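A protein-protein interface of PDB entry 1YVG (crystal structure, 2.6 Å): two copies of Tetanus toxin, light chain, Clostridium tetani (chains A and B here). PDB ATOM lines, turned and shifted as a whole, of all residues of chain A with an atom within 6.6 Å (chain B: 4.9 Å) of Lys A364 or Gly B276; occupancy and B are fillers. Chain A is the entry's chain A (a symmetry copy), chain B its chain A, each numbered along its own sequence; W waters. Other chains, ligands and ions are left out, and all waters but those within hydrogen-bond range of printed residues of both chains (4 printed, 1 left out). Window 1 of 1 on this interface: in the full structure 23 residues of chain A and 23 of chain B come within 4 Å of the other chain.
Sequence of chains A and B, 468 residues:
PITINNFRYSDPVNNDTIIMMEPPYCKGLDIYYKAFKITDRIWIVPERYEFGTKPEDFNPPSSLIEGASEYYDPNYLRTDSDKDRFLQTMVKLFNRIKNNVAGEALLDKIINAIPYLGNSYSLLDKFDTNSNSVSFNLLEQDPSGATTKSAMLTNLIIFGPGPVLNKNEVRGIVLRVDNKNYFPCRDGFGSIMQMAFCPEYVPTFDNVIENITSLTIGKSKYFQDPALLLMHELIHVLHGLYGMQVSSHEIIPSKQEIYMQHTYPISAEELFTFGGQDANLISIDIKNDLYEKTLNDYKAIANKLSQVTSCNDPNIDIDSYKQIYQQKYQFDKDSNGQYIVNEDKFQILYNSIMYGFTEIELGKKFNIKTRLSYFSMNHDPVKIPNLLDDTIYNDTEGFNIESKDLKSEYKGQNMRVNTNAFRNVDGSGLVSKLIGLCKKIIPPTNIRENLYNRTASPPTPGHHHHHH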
ATOM      1  N   LEU A 228     -14.084  -1.113 -11.278  1.00  0.00           N
ATOM      2  CA  LEU A 228     -13.395  -2.380 -11.527  1.00  0.00           C
ATOM      3  C   LEU A 228     -12.617  -2.234 -12.827  1.00  0.00           C
ATOM      4  O   LEU A 228     -11.532  -2.794 -12.975  1.00  0.00           O
ATOM      5  CB  LEU A 228     -14.384  -3.545 -11.648  1.00  0.00           C
ATOM      6  CG  LEU A 228     -13.741  -4.912 -11.938  1.00  0.00           C
ATOM      7  CD1 LEU A 228     -12.980  -5.390 -10.726  1.00  0.00           C
ATOM      8  CD2 LEU A 228     -14.794  -5.920 -12.302  1.00  0.00           C
ATOM      9  N   GLY A 276      -8.257 -16.092 -12.862  1.00  0.00           N
ATOM     10  CA  GLY A 276      -9.046 -17.307 -12.847  1.00  0.00           C
ATOM     11  C   GLY A 276      -8.428 -18.324 -13.786  1.00  0.00           C
ATOM     12  O   GLY A 276      -7.236 -18.252 -14.085  1.00  0.00           O
ATOM     13  N   GLN A 277      -9.227 -19.263 -14.274  1.00  0.00           N
ATOM     14  CA  GLN A 277      -8.702 -20.282 -15.168  1.00  0.00           C
ATOM     15  C   GLN A 277      -8.188 -19.733 -16.497  1.00  0.00           C
ATOM     16  O   GLN A 277      -7.347 -20.363 -17.131  1.00  0.00           O
ATOM     17  CB  GLN A 277      -9.757 -21.363 -15.415  1.00  0.00           C
ATOM     18  CG  GLN A 277     -10.076 -22.227 -14.196  1.00  0.00           C
ATOM     19  CD  GLN A 277      -9.075 -23.354 -13.968  1.00  0.00           C
ATOM     20  OE1 GLN A 277      -9.189 -24.109 -12.995  1.00  0.00           O
ATOM     21  NE2 GLN A 277      -8.101 -23.484 -14.868  1.00  0.00           N
ATOM     22  N   THR A 358      -5.794  -9.487  -9.814  1.00  0.00           N
ATOM     23  CA  THR A 358      -6.443  -9.825 -11.077  1.00  0.00           C
ATOM     24  C   THR A 358      -7.888  -9.353 -11.041  1.00  0.00           C
ATOM     25  O   THR A 358      -8.439  -9.137  -9.965  1.00  0.00           O
ATOM     26  CB  THR A 358      -6.436 -11.337 -11.316  1.00  0.00           C
ATOM     27  OG1 THR A 358      -7.246 -11.974 -10.323  1.00  0.00           O
ATOM     28  CG2 THR A 358      -5.019 -11.879 -11.237  1.00  0.00           C
ATOM     29  N   GLU A 359      -8.510  -9.200 -12.210  1.00  0.00           N
ATOM     30  CA  GLU A 359      -9.895  -8.735 -12.266  1.00  0.00           C
ATOM     31  C   GLU A 359     -10.856  -9.686 -11.548  1.00  0.00           C
ATOM     32  O   GLU A 359     -11.796  -9.254 -10.884  1.00  0.00           O
ATOM     33  CB  GLU A 359     -10.349  -8.539 -13.720  1.00  0.00           C
ATOM     34  CG  GLU A 359     -11.694  -7.794 -13.856  1.00  0.00           C
ATOM     35  CD  GLU A 359     -12.125  -7.557 -15.305  1.00  0.00           C
ATOM     36  OE1 GLU A 359     -11.313  -7.039 -16.106  1.00  0.00           O
ATOM     37  OE2 GLU A 359     -13.287  -7.882 -15.649  1.00  0.00           O
ATOM     38  N   ILE A 360     -10.615 -10.983 -11.676  1.00  0.00           N
ATOM     39  CA  ILE A 360     -11.463 -11.970 -11.034  1.00  0.00           C
ATOM     40  C   ILE A 360     -11.392 -11.917  -9.504  1.00  0.00           C
ATOM     41  O   ILE A 360     -12.412 -11.994  -8.815  1.00  0.00           O
ATOM     42  CB  ILE A 360     -11.094 -13.368 -11.523  1.00  0.00           C
ATOM     43  CG1 ILE A 360     -11.572 -13.518 -12.967  1.00  0.00           C
ATOM     44  CG2 ILE A 360     -11.664 -14.425 -10.593  1.00  0.00           C
ATOM     45  CD1 ILE A 360     -11.304 -14.874 -13.583  1.00  0.00           C
ATOM     46  N   GLU A 361     -10.189 -11.775  -8.967  1.00  0.00           N
ATOM     47  CA  GLU A 361     -10.051 -11.730  -7.530  1.00  0.00           C
ATOM     48  C   GLU A 361     -10.472 -10.386  -6.961  1.00  0.00           C
ATOM     49  O   GLU A 361     -10.992 -10.318  -5.851  1.00  0.00           O
ATOM     50  CB  GLU A 361      -8.617 -12.074  -7.131  1.00  0.00           C
ATOM     51  CG  GLU A 361      -8.242 -13.498  -7.486  1.00  0.00           C
ATOM     52  CD  GLU A 361      -9.326 -14.501  -7.102  1.00  0.00           C
ATOM     53  OE1 GLU A 361      -9.744 -14.504  -5.927  1.00  0.00           O
ATOM     54  OE2 GLU A 361      -9.758 -15.285  -7.974  1.00  0.00           O
ATOM     55  N   LEU A 362     -10.251  -9.313  -7.715  1.00  0.00           N
ATOM     56  CA  LEU A 362     -10.638  -7.998  -7.238  1.00  0.00           C
ATOM     57  C   LEU A 362     -12.148  -7.878  -7.302  1.00  0.00           C
ATOM     58  O   LEU A 362     -12.781  -7.323  -6.402  1.00  0.00           O
ATOM     59  CB  LEU A 362      -9.963  -6.909  -8.064  1.00  0.00           C
ATOM     60  CG  LEU A 362      -8.619  -6.508  -7.458  1.00  0.00           C
ATOM     61  CD1 LEU A 362      -7.786  -5.715  -8.435  1.00  0.00           C
ATOM     62  CD2 LEU A 362      -8.884  -5.713  -6.206  1.00  0.00           C
ATOM     63  N   GLY A 363     -12.728  -8.418  -8.365  1.00  0.00           N
ATOM     64  CA  GLY A 363     -14.169  -8.375  -8.490  1.00  0.00           C
ATOM     65  C   GLY A 363     -14.723  -9.119  -7.294  1.00  0.00           C
ATOM     66  O   GLY A 363     -15.663  -8.679  -6.630  1.00  0.00           O
ATOM     67  N   LYS A 364     -14.106 -10.256  -7.006  1.00  0.00           N
ATOM     68  CA  LYS A 364     -14.525 -11.081  -5.900  1.00  0.00           C
ATOM     69  C   LYS A 364     -14.496 -10.286  -4.594  1.00  0.00           C
ATOM     70  O   LYS A 364     -15.537 -10.100  -3.961  1.00  0.00           O
ATOM     71  CB  LYS A 364     -13.629 -12.309  -5.825  1.00  0.00           C
ATOM     72  CG  LYS A 364     -14.308 -13.517  -5.247  1.00  0.00           C
ATOM     73  CD  LYS A 364     -13.393 -14.715  -5.248  1.00  0.00           C
ATOM     74  CE  LYS A 364     -13.083 -15.197  -6.652  1.00  0.00           C
ATOM     75  NZ  LYS A 364     -12.270 -16.460  -6.612  1.00  0.00           N
ATOM     76  N   LYS A 365     -13.322  -9.791  -4.209  1.00  0.00           N
ATOM     77  CA  LYS A 365     -13.170  -9.020  -2.972  1.00  0.00           C
ATOM     78  C   LYS A 365     -13.930  -7.686  -2.931  1.00  0.00           C
ATOM     79  O   LYS A 365     -13.877  -6.977  -1.928  1.00  0.00           O
ATOM     80  CB  LYS A 365     -11.689  -8.749  -2.689  1.00  0.00           C
ATOM     81  CG  LYS A 365     -10.841  -9.976  -2.453  1.00  0.00           C
ATOM     82  CD  LYS A 365      -9.450  -9.552  -2.033  1.00  0.00           C
ATOM     83  CE  LYS A 365      -8.482 -10.714  -1.985  1.00  0.00           C
ATOM     84  NZ  LYS A 365      -8.221 -11.309  -3.339  1.00  0.00           N
ATOM     85  N   PHE A 366     -14.636  -7.351  -4.009  1.00  0.00           N
ATOM     86  CA  PHE A 366     -15.398  -6.100  -4.080  1.00  0.00           C
ATOM     87  C   PHE A 366     -16.928  -6.204  -4.189  1.00  0.00           C
ATOM     88  O   PHE A 366     -17.583  -5.191  -4.414  1.00  0.00           O
ATOM     89  CB  PHE A 366     -14.921  -5.255  -5.260  1.00  0.00           C
ATOM     90  CG  PHE A 366     -13.932  -4.190  -4.895  1.00  0.00           C
ATOM     91  CD1 PHE A 366     -12.578  -4.482  -4.786  1.00  0.00           C
ATOM     92  CD2 PHE A 366     -14.356  -2.878  -4.683  1.00  0.00           C
ATOM     93  CE1 PHE A 366     -11.662  -3.476  -4.474  1.00  0.00           C
ATOM     94  CE2 PHE A 366     -13.446  -1.866  -4.370  1.00  0.00           C
ATOM     95  CZ  PHE A 366     -12.100  -2.165  -4.267  1.00  0.00           C
ATOM     96  N   ASN A 367     -17.512  -7.389  -4.040  1.00  0.00           N
ATOM     97  CA  ASN A 367     -18.970  -7.501  -4.165  1.00  0.00           C
ATOM     98  C   ASN A 367     -19.346  -7.038  -5.586  1.00  0.00           C
ATOM     99  O   ASN A 367     -20.442  -6.537  -5.824  1.00  0.00           O
ATOM    100  CB  ASN A 367     -19.648  -6.648  -3.046  1.00  0.00           C
ATOM    101  CG  ASN A 367     -21.143  -6.263  -3.339  1.00  0.00           C
ATOM    102  OD1 ASN A 367     -21.952  -7.091  -3.804  1.00  0.00           O
ATOM    103  ND2 ASN A 367     -21.503  -4.995  -3.031  1.00  0.00           N
ATOM    104  N   ILE A 368     -18.425  -7.224  -6.532  1.00  0.00           N
ATOM    105  CA  ILE A 368     -18.655  -6.833  -7.926  1.00  0.00           C
ATOM    106  C   ILE A 368     -18.759  -8.033  -8.874  1.00  0.00           C
ATOM    107  O   ILE A 368     -17.988  -8.998  -8.785  1.00  0.00           O
ATOM    108  CB  ILE A 368     -17.534  -5.907  -8.446  1.00  0.00           C
ATOM    109  CG1 ILE A 368     -17.481  -4.629  -7.614  1.00  0.00           C
ATOM    110  CG2 ILE A 368     -17.775  -5.558  -9.910  1.00  0.00           C
ATOM    111  CD1 ILE A 368     -16.419  -3.667  -8.076  1.00  0.00           C
ATOM    112  N   THR A 370     -18.341 -10.150 -12.238  1.00  0.00           N
ATOM    113  CA  THR A 370     -17.333 -10.215 -13.293  1.00  0.00           C
ATOM    114  C   THR A 370     -17.895 -11.123 -14.385  1.00  0.00           C
ATOM    115  O   THR A 370     -18.790 -11.931 -14.109  1.00  0.00           O
ATOM    116  CB  THR A 370     -15.973 -10.820 -12.780  1.00  0.00           C
ATOM    117  OG1 THR A 370     -16.211 -12.043 -12.072  1.00  0.00           O
ATOM    118  CG2 THR A 370     -15.256  -9.845 -11.870  1.00  0.00           C
ATOM    119  N   TYR A 410     -25.787  -8.803  -6.631  1.00  0.00           N
ATOM    120  CA  TYR A 410     -25.225  -7.819  -7.545  1.00  0.00           C
ATOM    121  C   TYR A 410     -26.344  -7.180  -8.361  1.00  0.00           C
ATOM    122  O   TYR A 410     -26.109  -6.777  -9.503  1.00  0.00           O
ATOM    123  CB  TYR A 410     -24.254  -8.448  -8.565  1.00  0.00           C
ATOM    124  CG  TYR A 410     -23.273  -9.480  -8.054  1.00  0.00           C
ATOM    125  CD1 TYR A 410     -23.530 -10.839  -8.212  1.00  0.00           C
ATOM    126  CD2 TYR A 410     -22.069  -9.098  -7.447  1.00  0.00           C
ATOM    127  CE1 TYR A 410     -22.620 -11.795  -7.785  1.00  0.00           C
ATOM    128  CE2 TYR A 410     -21.146 -10.045  -7.014  1.00  0.00           C
ATOM    129  CZ  TYR A 410     -21.426 -11.397  -7.186  1.00  0.00           C
ATOM    130  OH  TYR A 410     -20.530 -12.358  -6.759  1.00  0.00           O
ATOM    131  N   PHE B 274     -11.919 -24.603  -3.443  1.00  0.00           N
ATOM    132  CA  PHE B 274     -11.532 -24.783  -4.841  1.00  0.00           C
ATOM    133  C   PHE B 274     -11.056 -23.446  -5.390  1.00  0.00           C
ATOM    134  O   PHE B 274      -9.903 -23.318  -5.800  1.00  0.00           O
ATOM    135  CB  PHE B 274     -12.690 -25.290  -5.696  1.00  0.00           C
ATOM    136  CG  PHE B 274     -12.254 -25.808  -7.041  1.00  0.00           C
ATOM    137  CD1 PHE B 274     -11.748 -27.096  -7.170  1.00  0.00           C
ATOM    138  CD2 PHE B 274     -12.326 -24.999  -8.171  1.00  0.00           C
ATOM    139  CE1 PHE B 274     -11.322 -27.568  -8.402  1.00  0.00           C
ATOM    140  CE2 PHE B 274     -11.901 -25.462  -9.408  1.00  0.00           C
ATOM    141  CZ  PHE B 274     -11.398 -26.745  -9.527  1.00  0.00           C
ATOM    142  N   GLY B 275     -11.957 -22.462  -5.398  1.00  0.00           N
ATOM    143  CA  GLY B 275     -11.617 -21.128  -5.865  1.00  0.00           C
ATOM    144  C   GLY B 275     -12.085 -20.759  -7.261  1.00  0.00           C
ATOM    145  O   GLY B 275     -13.061 -21.315  -7.777  1.00  0.00           O
ATOM    146  N   GLY B 276     -11.381 -19.813  -7.879  1.00  0.00           N
ATOM    147  CA  GLY B 276     -11.758 -19.383  -9.210  1.00  0.00           C
ATOM    148  C   GLY B 276     -13.202 -18.922  -9.204  1.00  0.00           C
ATOM    149  O   GLY B 276     -13.732 -18.549  -8.158  1.00  0.00           O
ATOM    150  N   GLN B 277     -13.856 -18.961 -10.357  1.00  0.00           N
ATOM    151  CA  GLN B 277     -15.238 -18.520 -10.433  1.00  0.00           C
ATOM    152  C   GLN B 277     -16.205 -19.374  -9.615  1.00  0.00           C
ATOM    153  O   GLN B 277     -17.266 -18.892  -9.228  1.00  0.00           O
ATOM    154  CB  GLN B 277     -15.694 -18.456 -11.893  1.00  0.00           C
ATOM    155  CG  GLN B 277     -15.026 -17.356 -12.717  1.00  0.00           C
ATOM    156  CD  GLN B 277     -15.660 -15.983 -12.532  1.00  0.00           C
ATOM    157  OE1 GLN B 277     -15.197 -14.993 -13.109  1.00  0.00           O
ATOM    158  NE2 GLN B 277     -16.730 -15.917 -11.739  1.00  0.00           N
ATOM    159  N   ASP B 278     -15.863 -20.627  -9.338  1.00  0.00           N
ATOM    160  CA  ASP B 278     -16.770 -21.459  -8.546  1.00  0.00           C
ATOM    161  C   ASP B 278     -17.009 -20.814  -7.182  1.00  0.00           C
ATOM    162  O   ASP B 278     -18.048 -21.015  -6.563  1.00  0.00           O
ATOM    163  CB  ASP B 278     -16.206 -22.874  -8.332  1.00  0.00           C
ATOM    164  CG  ASP B 278     -16.068 -23.659  -9.625  1.00  0.00           C
ATOM    165  OD1 ASP B 278     -15.165 -23.352 -10.438  1.00  0.00           O
ATOM    166  OD2 ASP B 278     -16.867 -24.592  -9.826  1.00  0.00           O
ATOM    167  N   ALA B 279     -16.037 -20.047  -6.708  1.00  0.00           N
ATOM    168  CA  ALA B 279     -16.175 -19.389  -5.417  1.00  0.00           C
ATOM    169  C   ALA B 279     -17.324 -18.393  -5.444  1.00  0.00           C
ATOM    170  O   ALA B 279     -17.966 -18.134  -4.425  1.00  0.00           O
ATOM    171  CB  ALA B 279     -14.884 -18.672  -5.052  1.00  0.00           C
ATOM    172  N   ASN B 280     -17.583 -17.835  -6.617  1.00  0.00           N
ATOM    173  CA  ASN B 280     -18.644 -16.862  -6.754  1.00  0.00           C
ATOM    174  C   ASN B 280     -20.037 -17.491  -6.819  1.00  0.00           C
ATOM    175  O   ASN B 280     -21.037 -16.787  -6.962  1.00  0.00           O
ATOM    176  CB  ASN B 280     -18.386 -15.997  -7.984  1.00  0.00           C
ATOM    177  CG  ASN B 280     -17.185 -15.084  -7.811  1.00  0.00           C
ATOM    178  OD1 ASN B 280     -16.679 -14.513  -8.778  1.00  0.00           O
ATOM    179  ND2 ASN B 280     -16.731 -14.934  -6.572  1.00  0.00           N
ATOM    180  N   LYS B 287     -22.114 -15.142   1.932  1.00  0.00           N
ATOM    181  CA  LYS B 287     -20.765 -14.650   2.152  1.00  0.00           C
ATOM    182  C   LYS B 287     -20.806 -13.545   3.177  1.00  0.00           C
ATOM    183  O   LYS B 287     -19.941 -13.445   4.041  1.00  0.00           O
ATOM    184  CB  LYS B 287     -20.166 -14.088   0.862  1.00  0.00           C
ATOM    185  CG  LYS B 287     -19.855 -15.096  -0.217  1.00  0.00           C
ATOM    186  CD  LYS B 287     -19.274 -14.364  -1.410  1.00  0.00           C
ATOM    187  CE  LYS B 287     -19.011 -15.278  -2.594  1.00  0.00           C
ATOM    188  NZ  LYS B 287     -18.656 -14.451  -3.782  1.00  0.00           N
ATOM    189  N   TYR B 355      -9.567 -16.542   0.740  1.00  0.00           N
ATOM    190  CA  TYR B 355      -9.182 -16.381  -0.658  1.00  0.00           C
ATOM    191  C   TYR B 355      -7.699 -16.582  -0.904  1.00  0.00           C
ATOM    192  O   TYR B 355      -7.299 -17.039  -1.966  1.00  0.00           O
ATOM    193  CB  TYR B 355      -9.612 -14.992  -1.161  1.00  0.00           C
ATOM    194  CG  TYR B 355     -11.097 -14.755  -1.026  1.00  0.00           C
ATOM    195  CD1 TYR B 355     -11.602 -13.853  -0.091  1.00  0.00           C
ATOM    196  CD2 TYR B 355     -12.006 -15.483  -1.797  1.00  0.00           C
ATOM    197  CE1 TYR B 355     -12.975 -13.684   0.077  1.00  0.00           C
ATOM    198  CE2 TYR B 355     -13.376 -15.327  -1.639  1.00  0.00           C
ATOM    199  CZ  TYR B 355     -13.862 -14.426  -0.698  1.00  0.00           C
ATOM    200  OH  TYR B 355     -15.232 -14.286  -0.535  1.00  0.00           O
ATOM    201  N   ILE B 360      -7.249 -23.728  -7.060  1.00  0.00           N
ATOM    202  CA  ILE B 360      -6.978 -23.129  -8.354  1.00  0.00           C
ATOM    203  C   ILE B 360      -5.704 -22.277  -8.364  1.00  0.00           C
ATOM    204  O   ILE B 360      -4.900 -22.345  -9.297  1.00  0.00           O
ATOM    205  CB  ILE B 360      -8.172 -22.286  -8.796  1.00  0.00           C
ATOM    206  CG1 ILE B 360      -9.313 -23.227  -9.182  1.00  0.00           C
ATOM    207  CG2 ILE B 360      -7.770 -21.343  -9.917  1.00  0.00           C
ATOM    208  CD1 ILE B 360     -10.563 -22.532  -9.675  1.00  0.00           C
HETATM  209  O   HOH W   1      -9.081 -16.707  -4.316  1.00  0.00           O
HETATM  210  O   HOH W   2     -17.919 -12.124  -5.909  1.00  0.00           O
HETATM  211  O   HOH W   3     -17.968 -11.059  -3.550  1.00  0.00           O
HETATM  212  O   HOH W   4     -14.832 -12.282  -9.459  1.00  0.00           O
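The side-chain amino group (NZ) of Lys A364 sits at hydrogen-bond distance from the backbone carbonyl oxygen (O) of Gly B276 (3.0 Å).
OE1 of Gln B277 lies within hydrogen-bond range of OG1 of Thr A370 (3.3 Å).
The backbone NH of Ile B360 is in hydrogen-bond range of the backbone carbonyl oxygen of Phe B274 (3.0 Å).
The side-chain amide nitrogen (NE2) of Gln B277 sits at hydrogen-bond distance from the side-chain amide oxygen (OD1) of Asn B280 (3.3 Å).
ND2 of Asn B280 lies close to NZ of Lys B287 (3.4 Å).
The side-chain carboxylate (OE2) of Glu A361 is in salt-bridge range of the side-chain amino group (NZ) of Lys A364 (3.1 Å).
CG1 of Ile B360 touches OE1 of Gln A277, 3.9 Å away.
Ile A360 touches Gln B277 (CG1 to OE1, 3.9 Å).
CB of Ala B279 touches NZ of Lys A364 (3.8 Å).
CG of Lys A364 touches ND2 of Asn B280, 3.1 Å away.
CD of Lys A364 touches CE2 of Tyr B355 (3.7 Å).
Printed residues of chain B within 4 Å of Ile A360: Gln B277.
Of the printed residues of chain B, Thr A370 touches Gln B277 (3.3 Å).
Gly B276 touches just one residue of chain A: Lys A364 (3.0 Å).
The nearest residue of chain B that does not touch Lys A364 is Gly B275 (4.4 Å).
Printed residues of chain A that touch a printed residue of chain B: Gln A277, Ile A360, Lys A364 and Thr A370.
Hydrophobic or aromatic side chains of chain A that line the printed part of chain B: Ile A360.
Along chain A the printed residues that touch a printed residue of chain B span positions 277 to 370.
Of the 10 printed residues of chain B, 6 touch a printed residue of chain A.
Among the printed residues, 7 pairs touch across the chains.
Gln A277 touches Ile B360, and with the chains exchanged Ile A360 touches Gln B277.
Of the 7 pairs that touch across the chains among the printed residues, 2 have their exchanged pair printed and touching as well.
Water W4 lies within hydrogen-bond range of the backbone carbonyl oxygen of Ile A360 (2.5 Å), the side-chain hydroxyl of Thr A370 (3.0 Å), the side-chain amide oxygen of Asn B280 (3.0 Å) and the backbone NH of Lys A364 (3.3 Å).
Water W3 lies within hydrogen-bond range of the backbone carbonyl oxygen of Lys A364 (2.6 Å) and the side-chain amino group of Lys B287 (3.5 Å).
Water W2 lies within hydrogen-bond range of OH of Tyr A410, ND2 of Asn B280 and NZ of Lys B287.
Water W1 lies within hydrogen-bond range of OE1 of Glu A361 (2.8 Å) and O of Tyr B355 (3.0 Å).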
